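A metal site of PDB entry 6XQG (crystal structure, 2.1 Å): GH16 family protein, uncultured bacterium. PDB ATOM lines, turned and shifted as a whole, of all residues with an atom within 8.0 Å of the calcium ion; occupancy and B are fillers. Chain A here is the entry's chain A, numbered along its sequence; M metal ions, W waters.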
ATOM      1  N   ASP A  30     -11.576  17.456 -24.365  1.00  0.00           N
ATOM      2  CA  ASP A  30     -12.553  18.054 -23.421  1.00  0.00           C
ATOM      3  C   ASP A  30     -13.381  16.879 -22.924  1.00  0.00           C
ATOM      4  O   ASP A  30     -14.211  16.339 -23.710  1.00  0.00           O
ATOM      5  CB  ASP A  30     -13.311  19.224 -24.025  1.00  0.00           C
ATOM      6  CG  ASP A  30     -13.880  20.132 -22.943  1.00  0.00           C
ATOM      7  OD1 ASP A  30     -13.979  19.653 -21.813  1.00  0.00           O
ATOM      8  OD2 ASP A  30     -14.289  21.253 -23.251  1.00  0.00           O
ATOM      9  N   GLU A  31     -13.028  16.398 -21.733  1.00  0.00           N
ATOM     10  CA  GLU A  31     -13.818  15.419 -20.951  1.00  0.00           C
ATOM     11  C   GLU A  31     -15.082  16.049 -20.373  1.00  0.00           C
ATOM     12  O   GLU A  31     -15.912  15.283 -19.894  1.00  0.00           O
ATOM     13  CB  GLU A  31     -12.963  14.841 -19.831  1.00  0.00           C
ATOM     14  CG  GLU A  31     -11.729  14.147 -20.349  1.00  0.00           C
ATOM     15  CD  GLU A  31     -11.948  12.859 -21.163  1.00  0.00           C
ATOM     16  OE1 GLU A  31     -13.077  12.315 -21.186  1.00  0.00           O
ATOM     17  OE2 GLU A  31     -10.911  12.365 -21.729  1.00  0.00           O
ATOM     18  N   PHE A  32     -15.223  17.390 -20.415  1.00  0.00           N
ATOM     19  CA  PHE A  32     -16.399  18.113 -19.852  1.00  0.00           C
ATOM     20  C   PHE A  32     -16.627  17.736 -18.376  1.00  0.00           C
ATOM     21  O   PHE A  32     -17.786  17.471 -17.953  1.00  0.00           O
ATOM     22  CB  PHE A  32     -17.660  17.842 -20.693  1.00  0.00           C
ATOM     23  CG  PHE A  32     -17.540  18.265 -22.119  1.00  0.00           C
ATOM     24  CD1 PHE A  32     -17.313  19.595 -22.439  1.00  0.00           C
ATOM     25  CD2 PHE A  32     -17.554  17.325 -23.140  1.00  0.00           C
ATOM     26  CE1 PHE A  32     -17.161  19.990 -23.771  1.00  0.00           C
ATOM     27  CE2 PHE A  32     -17.419  17.724 -24.457  1.00  0.00           C
ATOM     28  CZ  PHE A  32     -17.209  19.052 -24.770  1.00  0.00           C
ATOM     29  N   ASN A  33     -15.540  17.774 -17.604  1.00  0.00           N
ATOM     30  CA  ASN A  33     -15.504  17.412 -16.173  1.00  0.00           C
ATOM     31  C   ASN A  33     -16.110  18.532 -15.334  1.00  0.00           C
ATOM     32  O   ASN A  33     -16.581  18.217 -14.264  1.00  0.00           O
ATOM     33  CB  ASN A  33     -14.069  17.101 -15.715  1.00  0.00           C
ATOM     34  CG  ASN A  33     -13.530  15.880 -16.418  1.00  0.00           C
ATOM     35  OD1 ASN A  33     -14.318  15.032 -16.831  1.00  0.00           O
ATOM     36  ND2 ASN A  33     -12.216  15.780 -16.565  1.00  0.00           N
ATOM     37  N   THR A  34     -16.157  19.768 -15.830  1.00  0.00           N
ATOM     38  CA  THR A  34     -16.369  21.008 -15.016  1.00  0.00           C
ATOM     39  C   THR A  34     -17.729  21.599 -15.360  1.00  0.00           C
ATOM     40  O   THR A  34     -17.909  22.084 -16.476  1.00  0.00           O
ATOM     41  CB  THR A  34     -15.247  22.013 -15.270  1.00  0.00           C
ATOM     42  OG1 THR A  34     -14.022  21.398 -14.840  1.00  0.00           O
ATOM     43  CG2 THR A  34     -15.493  23.332 -14.589  1.00  0.00           C
ATOM     44  N   VAL A  72     -22.335  22.688 -19.593  1.00  0.00           N
ATOM     45  CA  VAL A  72     -21.626  21.421 -19.257  1.00  0.00           C
ATOM     46  C   VAL A  72     -22.316  20.921 -18.002  1.00  0.00           C
ATOM     47  O   VAL A  72     -22.359  21.695 -17.029  1.00  0.00           O
ATOM     48  CB  VAL A  72     -20.105  21.634 -19.061  1.00  0.00           C
ATOM     49  CG1 VAL A  72     -19.438  20.428 -18.428  1.00  0.00           C
ATOM     50  CG2 VAL A  72     -19.413  21.964 -20.358  1.00  0.00           C
ATOM     51  N   GLU A  73     -22.826  19.673 -18.042  1.00  0.00           N
ATOM     52  CA  GLU A  73     -23.765  19.120 -17.014  1.00  0.00           C
ATOM     53  C   GLU A  73     -23.566  17.599 -16.884  1.00  0.00           C
ATOM     54  O   GLU A  73     -23.606  16.893 -17.923  1.00  0.00           O
ATOM     55  CB  GLU A  73     -25.157  19.482 -17.506  1.00  0.00           C
ATOM     56  CG  GLU A  73     -26.184  19.673 -16.432  1.00  0.00           C
ATOM     57  CD  GLU A  73     -27.554  19.714 -17.061  1.00  0.00           C
ATOM     58  OE1 GLU A  73     -28.215  20.760 -16.999  1.00  0.00           O
ATOM     59  OE2 GLU A  73     -27.948  18.682 -17.605  1.00  0.00           O
ATOM     60  N   ASN A  74     -23.326  17.084 -15.661  1.00  0.00           N
ATOM     61  CA  ASN A  74     -23.181  15.628 -15.366  1.00  0.00           C
ATOM     62  C   ASN A  74     -22.182  14.948 -16.316  1.00  0.00           C
ATOM     63  O   ASN A  74     -22.424  13.837 -16.767  1.00  0.00           O
ATOM     64  CB  ASN A  74     -24.538  14.934 -15.446  1.00  0.00           C
ATOM     65  CG  ASN A  74     -25.488  15.534 -14.438  1.00  0.00           C
ATOM     66  OD1 ASN A  74     -26.657  15.789 -14.750  1.00  0.00           O
ATOM     67  ND2 ASN A  74     -24.971  15.839 -13.259  1.00  0.00           N
ATOM     68  N   GLY A  75     -21.069  15.622 -16.572  1.00  0.00           N
ATOM     69  CA  GLY A  75     -19.971  15.119 -17.422  1.00  0.00           C
ATOM     70  C   GLY A  75     -20.198  15.223 -18.920  1.00  0.00           C
ATOM     71  O   GLY A  75     -19.366  14.674 -19.661  1.00  0.00           O
ATOM     72  N   ASN A  76     -21.223  15.936 -19.380  1.00  0.00           N
ATOM     73  CA  ASN A  76     -21.526  16.112 -20.819  1.00  0.00           C
ATOM     74  C   ASN A  76     -21.625  17.585 -21.156  1.00  0.00           C
ATOM     75  O   ASN A  76     -22.153  18.380 -20.316  1.00  0.00           O
ATOM     76  CB  ASN A  76     -22.837  15.445 -21.231  1.00  0.00           C
ATOM     77  CG  ASN A  76     -22.887  13.970 -20.887  1.00  0.00           C
ATOM     78  OD1 ASN A  76     -21.981  13.210 -21.217  1.00  0.00           O
ATOM     79  ND2 ASN A  76     -23.951  13.576 -20.232  1.00  0.00           N
ATOM     80  N   LEU A  77     -21.141  17.935 -22.338  1.00  0.00           N
ATOM     81  CA  LEU A  77     -21.547  19.170 -23.018  1.00  0.00           C
ATOM     82  C   LEU A  77     -23.003  18.945 -23.407  1.00  0.00           C
ATOM     83  O   LEU A  77     -23.278  17.884 -24.021  1.00  0.00           O
ATOM     84  CB  LEU A  77     -20.712  19.392 -24.278  1.00  0.00           C
ATOM     85  CG  LEU A  77     -21.042  20.679 -25.042  1.00  0.00           C
ATOM     86  CD1 LEU A  77     -20.491  21.914 -24.293  1.00  0.00           C
ATOM     87  CD2 LEU A  77     -20.479  20.648 -26.460  1.00  0.00           C
ATOM     88  N   ARG A 118     -17.776  10.963 -28.236  1.00  0.00           N
ATOM     89  CA  ARG A 118     -18.785  10.063 -27.634  1.00  0.00           C
ATOM     90  C   ARG A 118     -20.002  10.925 -27.326  1.00  0.00           C
ATOM     91  O   ARG A 118     -19.796  12.002 -26.684  1.00  0.00           O
ATOM     92  CB  ARG A 118     -18.236   9.395 -26.365  1.00  0.00           C
ATOM     93  CG  ARG A 118     -19.171   8.365 -25.774  1.00  0.00           C
ATOM     94  CD  ARG A 118     -18.526   7.386 -24.802  1.00  0.00           C
ATOM     95  NE  ARG A 118     -19.522   6.397 -24.448  1.00  0.00           N
ATOM     96  CZ  ARG A 118     -20.318   6.425 -23.386  1.00  0.00           C
ATOM     97  NH1 ARG A 118     -20.236   7.372 -22.462  1.00  0.00           N
ATOM     98  NH2 ARG A 118     -21.242   5.470 -23.245  1.00  0.00           N
ATOM     99  N   PHE A 191     -25.395   6.600 -25.846  1.00  0.00           N
ATOM    100  CA  PHE A 191     -24.091   7.126 -26.313  1.00  0.00           C
ATOM    101  C   PHE A 191     -23.495   6.170 -27.351  1.00  0.00           C
ATOM    102  O   PHE A 191     -23.588   4.959 -27.157  1.00  0.00           O
ATOM    103  CB  PHE A 191     -23.113   7.291 -25.164  1.00  0.00           C
ATOM    104  CG  PHE A 191     -23.415   8.502 -24.343  1.00  0.00           C
ATOM    105  CD1 PHE A 191     -22.970   9.749 -24.757  1.00  0.00           C
ATOM    106  CD2 PHE A 191     -24.213   8.413 -23.231  1.00  0.00           C
ATOM    107  CE1 PHE A 191     -23.280  10.884 -24.015  1.00  0.00           C
ATOM    108  CE2 PHE A 191     -24.536   9.561 -22.515  1.00  0.00           C
ATOM    109  CZ  PHE A 191     -24.071  10.789 -22.913  1.00  0.00           C
ATOM    110  N   VAL A 260     -22.556  15.498 -25.360  1.00  0.00           N
ATOM    111  CA  VAL A 260     -21.156  15.087 -25.671  1.00  0.00           C
ATOM    112  C   VAL A 260     -20.429  14.776 -24.377  1.00  0.00           C
ATOM    113  O   VAL A 260     -20.018  15.747 -23.655  1.00  0.00           O
ATOM    114  CB  VAL A 260     -20.413  16.124 -26.489  1.00  0.00           C
ATOM    115  CG1 VAL A 260     -19.052  15.560 -26.880  1.00  0.00           C
ATOM    116  CG2 VAL A 260     -21.241  16.567 -27.708  1.00  0.00           C
ATOM    117  N   ASP A 261     -20.193  13.488 -24.162  1.00  0.00           N
ATOM    118  CA  ASP A 261     -19.471  12.958 -22.974  1.00  0.00           C
ATOM    119  C   ASP A 261     -18.012  13.387 -23.050  1.00  0.00           C
ATOM    120  O   ASP A 261     -17.498  13.861 -22.020  1.00  0.00           O
ATOM    121  CB  ASP A 261     -19.648  11.457 -22.868  1.00  0.00           C
ATOM    122  CG  ASP A 261     -18.870  10.774 -21.767  1.00  0.00           C
ATOM    123  OD1 ASP A 261     -18.425  11.462 -20.814  1.00  0.00           O
ATOM    124  OD2 ASP A 261     -18.715   9.542 -21.887  1.00  0.00           O
ATOM    125  N   TYR A 262     -17.391  13.271 -24.229  1.00  0.00           N
ATOM    126  CA  TYR A 262     -15.998  13.723 -24.431  1.00  0.00           C
ATOM    127  C   TYR A 262     -15.675  13.935 -25.903  1.00  0.00           C
ATOM    128  O   TYR A 262     -16.331  13.392 -26.828  1.00  0.00           O
ATOM    129  CB  TYR A 262     -15.004  12.740 -23.784  1.00  0.00           C
ATOM    130  CG  TYR A 262     -14.977  11.323 -24.297  1.00  0.00           C
ATOM    131  CD1 TYR A 262     -14.365  11.020 -25.497  1.00  0.00           C
ATOM    132  CD2 TYR A 262     -15.509  10.272 -23.556  1.00  0.00           C
ATOM    133  CE1 TYR A 262     -14.314   9.712 -25.955  1.00  0.00           C
ATOM    134  CE2 TYR A 262     -15.435   8.953 -23.991  1.00  0.00           C
ATOM    135  CZ  TYR A 262     -14.840   8.683 -25.194  1.00  0.00           C
ATOM    136  OH  TYR A 262     -14.756   7.426 -25.711  1.00  0.00           O
ATOM    137  N   VAL A 263     -14.651  14.765 -26.097  1.00  0.00           N
ATOM    138  CA  VAL A 263     -13.864  14.857 -27.342  1.00  0.00           C
ATOM    139  C   VAL A 263     -12.451  14.509 -26.927  1.00  0.00           C
ATOM    140  O   VAL A 263     -11.973  15.115 -25.955  1.00  0.00           O
ATOM    141  CB  VAL A 263     -13.915  16.248 -27.970  1.00  0.00           C
ATOM    142  CG1 VAL A 263     -13.014  16.307 -29.192  1.00  0.00           C
ATOM    143  CG2 VAL A 263     -15.323  16.667 -28.343  1.00  0.00           C
ATOM    144  N   ARG A 264     -11.845  13.564 -27.641  1.00  0.00           N
ATOM    145  CA  ARG A 264     -10.415  13.192 -27.515  1.00  0.00           C
ATOM    146  C   ARG A 264      -9.787  13.222 -28.908  1.00  0.00           C
ATOM    147  O   ARG A 264     -10.337  12.601 -29.820  1.00  0.00           O
ATOM    148  CB  ARG A 264     -10.304  11.804 -26.873  1.00  0.00           C
ATOM    149  CG  ARG A 264     -10.835  11.725 -25.450  1.00  0.00           C
ATOM    150  CD  ARG A 264     -10.782  10.300 -24.859  1.00  0.00           C
ATOM    151  NE  ARG A 264     -11.507  10.310 -23.605  1.00  0.00           N
ATOM    152  CZ  ARG A 264     -12.127   9.261 -23.080  1.00  0.00           C
ATOM    153  NH1 ARG A 264     -12.121   8.088 -23.698  1.00  0.00           N
ATOM    154  NH2 ARG A 264     -12.772   9.410 -21.946  1.00  0.00           N
HETATM  155 CA    CA M   1     -17.340  13.323 -19.726  1.00  0.00          CA
HETATM  156  O   HOH W   1     -15.311  12.124 -20.040  1.00  0.00           O
HETATM  157  O   HOH W   2     -18.632  12.047 -18.106  1.00  0.00           O
HETATM  158  O   HOH W   3     -16.565  13.845 -17.292  1.00  0.00           O
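The backbone carbonyl oxygen (O) of Glu 31 lies close to the side-chain amide oxygen (OD1) of Asn 33 (3.5 Å).
The side-chain carboxylate (OD2) of Asp 261 lies within salt-bridge range of the guanidinium group (NH1) of Arg 118, at 2.7 Å.
The backbone NH of Asp 261 lies close to the side-chain amide oxygen of Asn 76 (3.5 Å).
The guanidinium group (NE) of Arg 264 is in salt-bridge range of the side-chain carboxylate (OE2) of Glu 31, 2.8 Å away.
Three residues have an atom within 4 Å of the calcium ion: Glu 31, Gly 75 and Asp 261.
The nearest printed residue that does not touch the calcium ion is Tyr 262 (4.5 Å).
The calcium ion is bound by the backbone carbonyl oxygen of Asp 261 (2.4 Å), water W1 (2.4 Å), the side-chain carboxylate of Asp 261 (2.4 Å), the backbone carbonyl oxygen of Glu 31 (2.4 Å), water W2 (2.4 Å), the backbone carbonyl oxygen of Gly 75 (2.4 Å) and water W3 (2.6 Å).
The calcium ion has seven donor atoms within binding distance.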
